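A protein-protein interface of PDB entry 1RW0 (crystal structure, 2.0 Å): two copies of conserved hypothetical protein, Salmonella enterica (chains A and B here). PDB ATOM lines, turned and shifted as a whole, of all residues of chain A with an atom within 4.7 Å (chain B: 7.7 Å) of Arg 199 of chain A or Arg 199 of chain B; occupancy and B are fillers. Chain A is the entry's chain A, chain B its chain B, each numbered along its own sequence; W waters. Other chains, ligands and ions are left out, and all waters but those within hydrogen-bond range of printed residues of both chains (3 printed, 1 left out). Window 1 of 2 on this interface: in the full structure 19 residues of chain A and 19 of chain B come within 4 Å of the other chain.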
ATOM      1  N   LEU A 153      23.695 -24.554 -28.920  1.00  0.00           N
ATOM      2  CA  LEU A 153      24.775 -25.520 -29.104  1.00  0.00           C
ATOM      3  C   LEU A 153      24.335 -26.450 -30.232  1.00  0.00           C
ATOM      4  O   LEU A 153      23.318 -27.151 -30.113  1.00  0.00           O
ATOM      5  CB  LEU A 153      24.992 -26.319 -27.818  1.00  0.00           C
ATOM      6  CG  LEU A 153      25.217 -25.480 -26.553  1.00  0.00           C
ATOM      7  CD1 LEU A 153      25.434 -26.408 -25.359  1.00  0.00           C
ATOM      8  CD2 LEU A 153      26.428 -24.565 -26.739  1.00  0.00           C
ATOM      9  N   ASP A 193      32.684 -34.087 -22.440  1.00  0.00           N
ATOM     10  CA  ASP A 193      31.392 -33.500 -22.756  1.00  0.00           C
ATOM     11  C   ASP A 193      31.681 -32.095 -23.263  1.00  0.00           C
ATOM     12  O   ASP A 193      31.894 -31.170 -22.475  1.00  0.00           O
ATOM     13  CB  ASP A 193      30.495 -33.426 -21.519  1.00  0.00           C
ATOM     14  CG  ASP A 193      29.071 -33.041 -21.867  1.00  0.00           C
ATOM     15  OD1 ASP A 193      28.892 -32.283 -22.847  1.00  0.00           O
ATOM     16  OD2 ASP A 193      28.133 -33.485 -21.170  1.00  0.00           O
ATOM     17  N   TYR A 195      29.644 -30.161 -24.763  1.00  0.00           N
ATOM     18  CA  TYR A 195      28.509 -29.282 -24.486  1.00  0.00           C
ATOM     19  C   TYR A 195      28.660 -28.682 -23.087  1.00  0.00           C
ATOM     20  O   TYR A 195      28.464 -27.482 -22.886  1.00  0.00           O
ATOM     21  CB  TYR A 195      27.196 -30.062 -24.569  1.00  0.00           C
ATOM     22  CG  TYR A 195      26.923 -30.657 -25.927  1.00  0.00           C
ATOM     23  CD1 TYR A 195      26.713 -29.839 -27.038  1.00  0.00           C
ATOM     24  CD2 TYR A 195      26.885 -32.040 -26.107  1.00  0.00           C
ATOM     25  CE1 TYR A 195      26.472 -30.380 -28.296  1.00  0.00           C
ATOM     26  CE2 TYR A 195      26.645 -32.596 -27.364  1.00  0.00           C
ATOM     27  CZ  TYR A 195      26.439 -31.760 -28.453  1.00  0.00           C
ATOM     28  OH  TYR A 195      26.203 -32.303 -29.691  1.00  0.00           O
ATOM     29  N   GLN A 196      29.003 -29.530 -22.125  1.00  0.00           N
ATOM     30  CA  GLN A 196      29.205 -29.104 -20.742  1.00  0.00           C
ATOM     31  C   GLN A 196      30.318 -28.062 -20.669  1.00  0.00           C
ATOM     32  O   GLN A 196      30.205 -27.058 -19.964  1.00  0.00           O
ATOM     33  CB  GLN A 196      29.575 -30.311 -19.882  1.00  0.00           C
ATOM     34  CG  GLN A 196      29.568 -30.060 -18.373  1.00  0.00           C
ATOM     35  CD  GLN A 196      29.946 -31.308 -17.606  1.00  0.00           C
ATOM     36  OE1 GLN A 196      30.042 -32.390 -18.186  1.00  0.00           O
ATOM     37  NE2 GLN A 196      30.163 -31.173 -16.306  1.00  0.00           N
ATOM     38  N   LEU A 197      31.402 -28.301 -21.397  1.00  0.00           N
ATOM     39  CA  LEU A 197      32.516 -27.361 -21.401  1.00  0.00           C
ATOM     40  C   LEU A 197      32.085 -26.024 -22.014  1.00  0.00           C
ATOM     41  O   LEU A 197      32.459 -24.961 -21.523  1.00  0.00           O
ATOM     42  CB  LEU A 197      33.702 -27.949 -22.173  1.00  0.00           C
ATOM     43  CG  LEU A 197      34.358 -29.165 -21.503  1.00  0.00           C
ATOM     44  CD1 LEU A 197      35.336 -29.828 -22.461  1.00  0.00           C
ATOM     45  CD2 LEU A 197      35.066 -28.733 -20.231  1.00  0.00           C
ATOM     46  N   ALA A 198      31.285 -26.077 -23.076  1.00  0.00           N
ATOM     47  CA  ALA A 198      30.810 -24.856 -23.723  1.00  0.00           C
ATOM     48  C   ALA A 198      29.915 -24.076 -22.762  1.00  0.00           C
ATOM     49  O   ALA A 198      30.024 -22.852 -22.663  1.00  0.00           O
ATOM     50  CB  ALA A 198      30.040 -25.195 -25.012  1.00  0.00           C
ATOM     51  N   ARG A 199      29.026 -24.779 -22.060  1.00  0.00           N
ATOM     52  CA  ARG A 199      28.131 -24.118 -21.117  1.00  0.00           C
ATOM     53  C   ARG A 199      28.919 -23.470 -19.983  1.00  0.00           C
ATOM     54  O   ARG A 199      28.525 -22.417 -19.478  1.00  0.00           O
ATOM     55  CB  ARG A 199      27.092 -25.111 -20.569  1.00  0.00           C
ATOM     56  CG  ARG A 199      26.006 -25.468 -21.598  1.00  0.00           C
ATOM     57  CD  ARG A 199      24.898 -26.365 -21.037  1.00  0.00           C
ATOM     58  NE  ARG A 199      25.281 -27.775 -21.041  1.00  0.00           N
ATOM     59  CZ  ARG A 199      24.738 -28.702 -21.822  1.00  0.00           C
ATOM     60  NH1 ARG A 199      23.773 -28.392 -22.674  1.00  0.00           N
ATOM     61  NH2 ARG A 199      25.171 -29.947 -21.758  1.00  0.00           N
ATOM     62  N   GLN A 200      30.029 -24.096 -19.594  1.00  0.00           N
ATOM     63  CA  GLN A 200      30.899 -23.568 -18.540  1.00  0.00           C
ATOM     64  C   GLN A 200      31.549 -22.255 -18.967  1.00  0.00           C
ATOM     65  O   GLN A 200      31.508 -21.259 -18.239  1.00  0.00           O
ATOM     66  CB  GLN A 200      32.018 -24.562 -18.206  1.00  0.00           C
ATOM     67  CG  GLN A 200      31.632 -25.690 -17.269  1.00  0.00           C
ATOM     68  CD  GLN A 200      32.773 -26.669 -17.054  1.00  0.00           C
ATOM     69  OE1 GLN A 200      33.915 -26.403 -17.437  1.00  0.00           O
ATOM     70  NE2 GLN A 200      32.471 -27.805 -16.429  1.00  0.00           N
ATOM     71  N   ARG A 201      32.160 -22.255 -20.148  1.00  0.00           N
ATOM     72  CA  ARG A 201      32.827 -21.053 -20.633  1.00  0.00           C
ATOM     73  C   ARG A 201      31.821 -19.935 -20.925  1.00  0.00           C
ATOM     74  O   ARG A 201      32.093 -18.760 -20.662  1.00  0.00           O
ATOM     75  CB  ARG A 201      33.685 -21.389 -21.866  1.00  0.00           C
ATOM     76  CG  ARG A 201      34.730 -22.515 -21.617  1.00  0.00           C
ATOM     77  CD  ARG A 201      35.618 -22.250 -20.371  1.00  0.00           C
ATOM     78  NE  ARG A 201      36.758 -23.176 -20.233  1.00  0.00           N
ATOM     79  CZ  ARG A 201      36.839 -24.194 -19.360  1.00  0.00           C
ATOM     80  NH1 ARG A 201      35.842 -24.454 -18.510  1.00  0.00           N
ATOM     81  NH2 ARG A 201      37.942 -24.960 -19.322  1.00  0.00           N
ATOM     82  N   LEU A 202      30.652 -20.290 -21.452  1.00  0.00           N
ATOM     83  CA  LEU A 202      29.635 -19.283 -21.722  1.00  0.00           C
ATOM     84  C   LEU A 202      29.167 -18.686 -20.397  1.00  0.00           C
ATOM     85  O   LEU A 202      28.982 -17.473 -20.285  1.00  0.00           O
ATOM     86  CB  LEU A 202      28.455 -19.901 -22.477  1.00  0.00           C
ATOM     87  CG  LEU A 202      28.770 -20.241 -23.942  1.00  0.00           C
ATOM     88  CD1 LEU A 202      27.678 -21.118 -24.546  1.00  0.00           C
ATOM     89  CD2 LEU A 202      28.917 -18.953 -24.725  1.00  0.00           C
ATOM     90  N   ALA A 203      28.986 -19.541 -19.393  1.00  0.00           N
ATOM     91  CA  ALA A 203      28.545 -19.091 -18.079  1.00  0.00           C
ATOM     92  C   ALA A 203      29.597 -18.197 -17.426  1.00  0.00           C
ATOM     93  O   ALA A 203      29.262 -17.302 -16.650  1.00  0.00           O
ATOM     94  CB  ALA A 203      28.243 -20.283 -17.190  1.00  0.00           C
ATOM     95  N   VAL A 210      21.441 -20.878 -22.675  1.00  0.00           N
ATOM     96  CA  VAL A 210      22.113 -21.729 -23.654  1.00  0.00           C
ATOM     97  C   VAL A 210      21.171 -22.876 -24.022  1.00  0.00           C
ATOM     98  O   VAL A 210      20.681 -23.581 -23.145  1.00  0.00           O
ATOM     99  CB  VAL A 210      23.429 -22.309 -23.075  1.00  0.00           C
ATOM    100  CG1 VAL A 210      24.173 -23.099 -24.151  1.00  0.00           C
ATOM    101  CG2 VAL A 210      24.308 -21.178 -22.538  1.00  0.00           C
ATOM    102  N   GLY A 212      19.980 -26.148 -27.121  1.00  0.00           N
ATOM    103  CA  GLY A 212      20.556 -27.183 -27.964  1.00  0.00           C
ATOM    104  C   GLY A 212      21.465 -28.104 -27.174  1.00  0.00           C
ATOM    105  O   GLY A 212      21.448 -28.086 -25.948  1.00  0.00           O
ATOM    106  N   LEU B 108      10.047 -33.946 -16.760  1.00  0.00           N
ATOM    107  CA  LEU B 108      11.378 -34.486 -16.921  1.00  0.00           C
ATOM    108  C   LEU B 108      11.659 -35.825 -16.270  1.00  0.00           C
ATOM    109  O   LEU B 108      11.560 -35.961 -15.060  1.00  0.00           O
ATOM    110  CB  LEU B 108      12.396 -33.476 -16.395  1.00  0.00           C
ATOM    111  CG  LEU B 108      13.861 -33.897 -16.400  1.00  0.00           C
ATOM    112  CD1 LEU B 108      14.350 -34.085 -17.836  1.00  0.00           C
ATOM    113  CD2 LEU B 108      14.681 -32.824 -15.685  1.00  0.00           C
ATOM    114  N   LEU B 130      10.833 -31.220  -8.977  1.00  0.00           N
ATOM    115  CA  LEU B 130      12.191 -30.780  -9.254  1.00  0.00           C
ATOM    116  C   LEU B 130      12.553 -29.666  -8.272  1.00  0.00           C
ATOM    117  O   LEU B 130      13.630 -29.679  -7.667  1.00  0.00           O
ATOM    118  CB  LEU B 130      12.298 -30.269 -10.691  1.00  0.00           C
ATOM    119  CG  LEU B 130      13.690 -29.792 -11.123  1.00  0.00           C
ATOM    120  CD1 LEU B 130      14.703 -30.894 -10.890  1.00  0.00           C
ATOM    121  CD2 LEU B 130      13.663 -29.396 -12.591  1.00  0.00           C
ATOM    122  N   LEU B 135      15.283 -34.825  -7.208  1.00  0.00           N
ATOM    123  CA  LEU B 135      16.541 -35.334  -7.735  1.00  0.00           C
ATOM    124  C   LEU B 135      17.565 -35.486  -6.614  1.00  0.00           C
ATOM    125  O   LEU B 135      18.308 -36.466  -6.588  1.00  0.00           O
ATOM    126  CB  LEU B 135      17.087 -34.419  -8.840  1.00  0.00           C
ATOM    127  CG  LEU B 135      16.162 -34.215 -10.048  1.00  0.00           C
ATOM    128  CD1 LEU B 135      16.888 -33.398 -11.113  1.00  0.00           C
ATOM    129  CD2 LEU B 135      15.742 -35.571 -10.621  1.00  0.00           C
ATOM    130  N   LEU B 153      19.063 -37.327 -18.708  1.00  0.00           N
ATOM    131  CA  LEU B 153      17.855 -36.510 -18.759  1.00  0.00           C
ATOM    132  C   LEU B 153      17.019 -36.964 -19.954  1.00  0.00           C
ATOM    133  O   LEU B 153      17.461 -36.861 -21.098  1.00  0.00           O
ATOM    134  CB  LEU B 153      18.224 -35.029 -18.913  1.00  0.00           C
ATOM    135  CG  LEU B 153      19.170 -34.440 -17.853  1.00  0.00           C
ATOM    136  CD1 LEU B 153      19.479 -32.986 -18.197  1.00  0.00           C
ATOM    137  CD2 LEU B 153      18.524 -34.524 -16.473  1.00  0.00           C
ATOM    138  N   ASP B 193      13.828 -23.505 -18.743  1.00  0.00           N
ATOM    139  CA  ASP B 193      14.628 -24.618 -19.239  1.00  0.00           C
ATOM    140  C   ASP B 193      14.702 -25.634 -18.106  1.00  0.00           C
ATOM    141  O   ASP B 193      15.501 -25.485 -17.185  1.00  0.00           O
ATOM    142  CB  ASP B 193      16.037 -24.142 -19.584  1.00  0.00           C
ATOM    143  CG  ASP B 193      16.872 -25.222 -20.254  1.00  0.00           C
ATOM    144  OD1 ASP B 193      16.697 -26.418 -19.928  1.00  0.00           O
ATOM    145  OD2 ASP B 193      17.716 -24.872 -21.098  1.00  0.00           O
ATOM    146  N   ILE B 194      13.865 -26.661 -18.173  1.00  0.00           N
ATOM    147  CA  ILE B 194      13.839 -27.678 -17.130  1.00  0.00           C
ATOM    148  C   ILE B 194      15.148 -28.473 -17.070  1.00  0.00           C
ATOM    149  O   ILE B 194      15.533 -28.972 -16.010  1.00  0.00           O
ATOM    150  CB  ILE B 194      12.646 -28.635 -17.339  1.00  0.00           C
ATOM    151  CG1 ILE B 194      12.423 -29.468 -16.079  1.00  0.00           C
ATOM    152  CG2 ILE B 194      12.897 -29.540 -18.542  1.00  0.00           C
ATOM    153  CD1 ILE B 194      11.159 -30.305 -16.131  1.00  0.00           C
ATOM    154  N   TYR B 195      15.840 -28.587 -18.200  1.00  0.00           N
ATOM    155  CA  TYR B 195      17.100 -29.323 -18.225  1.00  0.00           C
ATOM    156  C   TYR B 195      18.186 -28.580 -17.460  1.00  0.00           C
ATOM    157  O   TYR B 195      18.958 -29.186 -16.709  1.00  0.00           O
ATOM    158  CB  TYR B 195      17.545 -29.541 -19.663  1.00  0.00           C
ATOM    159  CG  TYR B 195      16.515 -30.248 -20.508  1.00  0.00           C
ATOM    160  CD1 TYR B 195      16.129 -31.555 -20.219  1.00  0.00           C
ATOM    161  CD2 TYR B 195      15.945 -29.619 -21.611  1.00  0.00           C
ATOM    162  CE1 TYR B 195      15.198 -32.229 -21.016  1.00  0.00           C
ATOM    163  CE2 TYR B 195      15.012 -30.281 -22.415  1.00  0.00           C
ATOM    164  CZ  TYR B 195      14.650 -31.586 -22.109  1.00  0.00           C
ATOM    165  OH  TYR B 195      13.759 -32.252 -22.912  1.00  0.00           O
ATOM    166  N   GLN B 196      18.251 -27.269 -17.672  1.00  0.00           N
ATOM    167  CA  GLN B 196      19.224 -26.418 -16.995  1.00  0.00           C
ATOM    168  C   GLN B 196      18.977 -26.505 -15.491  1.00  0.00           C
ATOM    169  O   GLN B 196      19.913 -26.606 -14.701  1.00  0.00           O
ATOM    170  CB  GLN B 196      19.063 -24.971 -17.473  1.00  0.00           C
ATOM    171  CG  GLN B 196      20.073 -23.981 -16.924  1.00  0.00           C
ATOM    172  CD  GLN B 196      19.880 -22.592 -17.514  1.00  0.00           C
ATOM    173  OE1 GLN B 196      18.985 -22.373 -18.332  1.00  0.00           O
ATOM    174  NE2 GLN B 196      20.716 -21.650 -17.102  1.00  0.00           N
ATOM    175  N   LEU B 197      17.710 -26.462 -15.099  1.00  0.00           N
ATOM    176  CA  LEU B 197      17.367 -26.554 -13.687  1.00  0.00           C
ATOM    177  C   LEU B 197      17.810 -27.901 -13.132  1.00  0.00           C
ATOM    178  O   LEU B 197      18.364 -27.973 -12.036  1.00  0.00           O
ATOM    179  CB  LEU B 197      15.862 -26.351 -13.492  1.00  0.00           C
ATOM    180  CG  LEU B 197      15.455 -24.883 -13.671  1.00  0.00           C
ATOM    181  CD1 LEU B 197      13.956 -24.766 -13.767  1.00  0.00           C
ATOM    182  CD2 LEU B 197      15.986 -24.057 -12.512  1.00  0.00           C
ATOM    183  N   ALA B 198      17.594 -28.967 -13.900  1.00  0.00           N
ATOM    184  CA  ALA B 198      18.002 -30.297 -13.453  1.00  0.00           C
ATOM    185  C   ALA B 198      19.524 -30.383 -13.327  1.00  0.00           C
ATOM    186  O   ALA B 198      20.042 -30.976 -12.377  1.00  0.00           O
ATOM    187  CB  ALA B 198      17.496 -31.364 -14.424  1.00  0.00           C
ATOM    188  N   ARG B 199      20.247 -29.804 -14.284  1.00  0.00           N
ATOM    189  CA  ARG B 199      21.704 -29.850 -14.221  1.00  0.00           C
ATOM    190  C   ARG B 199      22.230 -29.063 -13.013  1.00  0.00           C
ATOM    191  O   ARG B 199      23.230 -29.443 -12.398  1.00  0.00           O
ATOM    192  CB  ARG B 199      22.318 -29.332 -15.533  1.00  0.00           C
ATOM    193  CG  ARG B 199      22.095 -30.288 -16.714  1.00  0.00           C
ATOM    194  CD  ARG B 199      22.927 -29.916 -17.934  1.00  0.00           C
ATOM    195  NE  ARG B 199      22.361 -28.799 -18.678  1.00  0.00           N
ATOM    196  CZ  ARG B 199      21.661 -28.924 -19.803  1.00  0.00           C
ATOM    197  NH1 ARG B 199      21.436 -30.122 -20.326  1.00  0.00           N
ATOM    198  NH2 ARG B 199      21.187 -27.845 -20.406  1.00  0.00           N
ATOM    199  N   GLN B 200      21.547 -27.977 -12.668  1.00  0.00           N
ATOM    200  CA  GLN B 200      21.940 -27.169 -11.515  1.00  0.00           C
ATOM    201  C   GLN B 200      21.801 -27.982 -10.232  1.00  0.00           C
ATOM    202  O   GLN B 200      22.741 -28.095  -9.440  1.00  0.00           O
ATOM    203  CB  GLN B 200      21.060 -25.921 -11.399  1.00  0.00           C
ATOM    204  CG  GLN B 200      21.463 -24.770 -12.299  1.00  0.00           C
ATOM    205  CD  GLN B 200      20.531 -23.575 -12.170  1.00  0.00           C
ATOM    206  OE1 GLN B 200      19.843 -23.412 -11.157  1.00  0.00           O
ATOM    207  NE2 GLN B 200      20.508 -22.728 -13.199  1.00  0.00           N
ATOM    208  N   ARG B 201      20.616 -28.546 -10.028  1.00  0.00           N
ATOM    209  CA  ARG B 201      20.367 -29.331  -8.836  1.00  0.00           C
ATOM    210  C   ARG B 201      21.294 -30.539  -8.775  1.00  0.00           C
ATOM    211  O   ARG B 201      21.841 -30.855  -7.715  1.00  0.00           O
ATOM    212  CB  ARG B 201      18.892 -29.763  -8.782  1.00  0.00           C
ATOM    213  CG  ARG B 201      17.900 -28.584  -8.687  1.00  0.00           C
ATOM    214  CD  ARG B 201      18.253 -27.636  -7.531  1.00  0.00           C
ATOM    215  NE  ARG B 201      17.273 -26.560  -7.329  1.00  0.00           N
ATOM    216  CZ  ARG B 201      17.313 -25.357  -7.912  1.00  0.00           C
ATOM    217  NH1 ARG B 201      18.288 -25.040  -8.757  1.00  0.00           N
ATOM    218  NH2 ARG B 201      16.373 -24.452  -7.635  1.00  0.00           N
ATOM    219  N   LEU B 202      21.491 -31.209  -9.906  1.00  0.00           N
ATOM    220  CA  LEU B 202      22.370 -32.373  -9.928  1.00  0.00           C
ATOM    221  C   LEU B 202      23.805 -31.994  -9.549  1.00  0.00           C
ATOM    222  O   LEU B 202      24.453 -32.687  -8.760  1.00  0.00           O
ATOM    223  CB  LEU B 202      22.323 -33.043 -11.306  1.00  0.00           C
ATOM    224  CG  LEU B 202      21.022 -33.811 -11.583  1.00  0.00           C
ATOM    225  CD1 LEU B 202      20.938 -34.223 -13.047  1.00  0.00           C
ATOM    226  CD2 LEU B 202      20.963 -35.036 -10.684  1.00  0.00           C
ATOM    227  N   ALA B 203      24.299 -30.885 -10.090  1.00  0.00           N
ATOM    228  CA  ALA B 203      25.650 -30.437  -9.766  1.00  0.00           C
ATOM    229  C   ALA B 203      25.753 -30.189  -8.256  1.00  0.00           C
ATOM    230  O   ALA B 203      26.758 -30.544  -7.627  1.00  0.00           O
ATOM    231  CB  ALA B 203      25.972 -29.162 -10.533  1.00  0.00           C
ATOM    232  N   ASN B 204      24.705 -29.589  -7.690  1.00  0.00           N
ATOM    233  CA  ASN B 204      24.637 -29.283  -6.254  1.00  0.00           C
ATOM    234  C   ASN B 204      24.892 -30.496  -5.368  1.00  0.00           C
ATOM    235  O   ASN B 204      25.474 -30.368  -4.293  1.00  0.00           O
ATOM    236  CB  ASN B 204      23.260 -28.719  -5.876  1.00  0.00           C
ATOM    237  CG  ASN B 204      23.061 -27.282  -6.323  1.00  0.00           C
ATOM    238  OD1 ASN B 204      23.968 -26.648  -6.861  1.00  0.00           O
ATOM    239  ND2 ASN B 204      21.860 -26.759  -6.091  1.00  0.00           N
ATOM    240  N   THR B 205      24.436 -31.665  -5.816  1.00  0.00           N
ATOM    241  CA  THR B 205      24.594 -32.907  -5.058  1.00  0.00           C
ATOM    242  C   THR B 205      25.955 -33.551  -5.260  1.00  0.00           C
ATOM    243  O   THR B 205      26.331 -34.463  -4.527  1.00  0.00           O
ATOM    244  CB  THR B 205      23.538 -33.951  -5.460  1.00  0.00           C
ATOM    245  OG1 THR B 205      23.762 -34.354  -6.814  1.00  0.00           O
ATOM    246  CG2 THR B 205      22.146 -33.381  -5.329  1.00  0.00           C
ATOM    247  N   VAL B 207      26.891 -34.715  -8.404  1.00  0.00           N
ATOM    248  CA  VAL B 207      26.847 -35.482  -9.644  1.00  0.00           C
ATOM    249  C   VAL B 207      27.526 -34.613 -10.696  1.00  0.00           C
ATOM    250  O   VAL B 207      27.240 -33.419 -10.795  1.00  0.00           O
ATOM    251  CB  VAL B 207      25.385 -35.789 -10.072  1.00  0.00           C
ATOM    252  CG1 VAL B 207      25.363 -36.412 -11.462  1.00  0.00           C
ATOM    253  CG2 VAL B 207      24.746 -36.748  -9.072  1.00  0.00           C
ATOM    254  N   GLU B 208      28.427 -35.204 -11.473  1.00  0.00           N
ATOM    255  CA  GLU B 208      29.165 -34.455 -12.485  1.00  0.00           C
ATOM    256  C   GLU B 208      28.781 -34.745 -13.931  1.00  0.00           C
ATOM    257  O   GLU B 208      28.695 -33.834 -14.754  1.00  0.00           O
ATOM    258  CB  GLU B 208      30.667 -34.713 -12.324  1.00  0.00           C
ATOM    259  CG  GLU B 208      31.229 -34.333 -10.965  1.00  0.00           C
ATOM    260  CD  GLU B 208      32.707 -34.653 -10.829  1.00  0.00           C
ATOM    261  OE1 GLU B 208      33.247 -34.489  -9.719  1.00  0.00           O
ATOM    262  OE2 GLU B 208      33.333 -35.068 -11.829  1.00  0.00           O
ATOM    263  N   VAL B 210      26.173 -35.665 -16.602  1.00  0.00           N
ATOM    264  CA  VAL B 210      24.752 -35.716 -16.928  1.00  0.00           C
ATOM    265  C   VAL B 210      24.642 -35.789 -18.444  1.00  0.00           C
ATOM    266  O   VAL B 210      25.291 -35.016 -19.160  1.00  0.00           O
ATOM    267  CB  VAL B 210      24.017 -34.463 -16.396  1.00  0.00           C
ATOM    268  CG1 VAL B 210      22.517 -34.560 -16.690  1.00  0.00           C
ATOM    269  CG2 VAL B 210      24.245 -34.336 -14.898  1.00  0.00           C
ATOM    270  N   TYR B 211      23.827 -36.724 -18.922  1.00  0.00           N
ATOM    271  CA  TYR B 211      23.638 -36.962 -20.351  1.00  0.00           C
ATOM    272  C   TYR B 211      22.223 -36.638 -20.811  1.00  0.00           C
ATOM    273  O   TYR B 211      21.340 -36.365 -19.997  1.00  0.00           O
ATOM    274  CB  TYR B 211      23.958 -38.432 -20.656  1.00  0.00           C
ATOM    275  CG  TYR B 211      25.354 -38.819 -20.243  1.00  0.00           C
ATOM    276  CD1 TYR B 211      26.415 -38.749 -21.150  1.00  0.00           C
ATOM    277  CD2 TYR B 211      25.639 -39.167 -18.921  1.00  0.00           C
ATOM    278  CE1 TYR B 211      27.724 -39.004 -20.748  1.00  0.00           C
ATOM    279  CE2 TYR B 211      26.944 -39.425 -18.508  1.00  0.00           C
ATOM    280  CZ  TYR B 211      27.980 -39.336 -19.424  1.00  0.00           C
ATOM    281  OH  TYR B 211      29.279 -39.537 -19.014  1.00  0.00           O
ATOM    282  N   GLY B 212      22.008 -36.664 -22.121  1.00  0.00           N
ATOM    283  CA  GLY B 212      20.690 -36.364 -22.649  1.00  0.00           C
ATOM    284  C   GLY B 212      20.325 -34.895 -22.534  1.00  0.00           C
ATOM    285  O   GLY B 212      21.203 -34.030 -22.582  1.00  0.00           O
ATOM    286  N   GLY B 213      19.030 -34.616 -22.361  1.00  0.00           N
ATOM    287  CA  GLY B 213      18.552 -33.244 -22.258  1.00  0.00           C
ATOM    288  C   GLY B 213      18.243 -32.822 -23.673  1.00  0.00           C
ATOM    289  O   GLY B 213      17.908 -31.677 -23.984  1.00  0.00           O
ATOM    290  N   ASP B 214      18.348 -33.836 -24.516  1.00  0.00           N
ATOM    291  CA  ASP B 214      18.168 -33.811 -25.952  1.00  0.00           C
ATOM    292  C   ASP B 214      16.768 -33.776 -26.582  1.00  0.00           C
ATOM    293  O   ASP B 214      16.609 -34.281 -27.692  1.00  0.00           O
ATOM    294  CB  ASP B 214      18.892 -35.034 -26.518  1.00  0.00           C
ATOM    295  CG  ASP B 214      18.430 -36.328 -25.869  1.00  0.00           C
ATOM    296  OD1 ASP B 214      18.870 -37.410 -26.313  1.00  0.00           O
ATOM    297  OD2 ASP B 214      17.622 -36.264 -24.913  1.00  0.00           O
HETATM  298  O   HOH W   1      23.603 -31.994 -23.660  1.00  0.00           O
HETATM  299  O   HOH W   2      19.575 -26.594 -21.963  1.00  0.00           O
HETATM  300  O   HOH W   3      28.408 -35.478 -19.512  1.00  0.00           O
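The guanidinium group of Arg 199 of chain B lies close to the guanidinium group of Arg 199 of chain A, at 3.5 Å.
NE2 of Gln 196 of chain A sits at hydrogen-bond distance from O of Glu 208 of chain B, at 3.4 Å.
The side-chain carboxylate (OD1) of Asp 193 of chain A sits at hydrogen-bond distance from the backbone NH (N) of Tyr 195 of chain A (3.0 Å).
OD1 of Asp 193 of chain B lies within hydrogen-bond range of N of Tyr 195 of chain B (2.9 Å).
The side-chain carboxylate of Asp 193 of chain B is in hydrogen-bond range of the backbone NH of Gln 196 of chain B (2.9 Å).
The backbone NH of Gln 196 of chain A is in hydrogen-bond range of the side-chain carboxylate of Asp 193 of chain A, at 2.8 Å.
Val 210 of chain B touches Asp 193 of chain A.
O of Val 210 of chain A touches OD2 of Asp 193 of chain B, at 3.8 Å.
Arg 199 of chain A touches just one residue of chain B: Arg 199 (3.5 Å).
Of chain A, only Arg 199 (3.5 Å) comes within 4 Å of Arg 199 of chain B.
No residue of chain B comes within 4 Å of Ala 198 of chain A.
Of the printed residues of chain B, Val 210 of chain A touches Asp 193 (3.8 Å).
Of the printed residues of chain B, Gln 196 of chain A touches Glu 208 (3.4 Å).
Ile 194 of chain B touches none of the printed residues of chain A.
Gln 200 of chain B touches none of the printed residues of chain A.
The nearest printed residue of chain A that does not touch Arg 199 of chain B is Val 210 of chain A (5.1 Å).
The nearest printed residue of chain A that does not touch Asp 193 of chain B is Gly 212 of chain A (6.6 Å).
Asp 193 of chain A touches Val 210 of chain B, and with the chains exchanged Val 210 of chain A touches Asp 193 of chain B.
Arg 199 of chain A touches its own counterpart, Arg 199 of chain B.
Water W2 lies within hydrogen-bond range of NH2 of Arg 199 of chain B (2.6 Å), OD2 of Asp 193 of chain B (2.7 Å) and O of Val 210 of chain A (3.4 Å).
Water W3 lies within hydrogen-bond range of OD2 of Asp 193 of chain A and O of Val 210 of chain B.
Water W1 bridges NH2 of Arg 199 of chain A (3.2 Å) and O of Gly 212 of chain B (3.3 Å).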
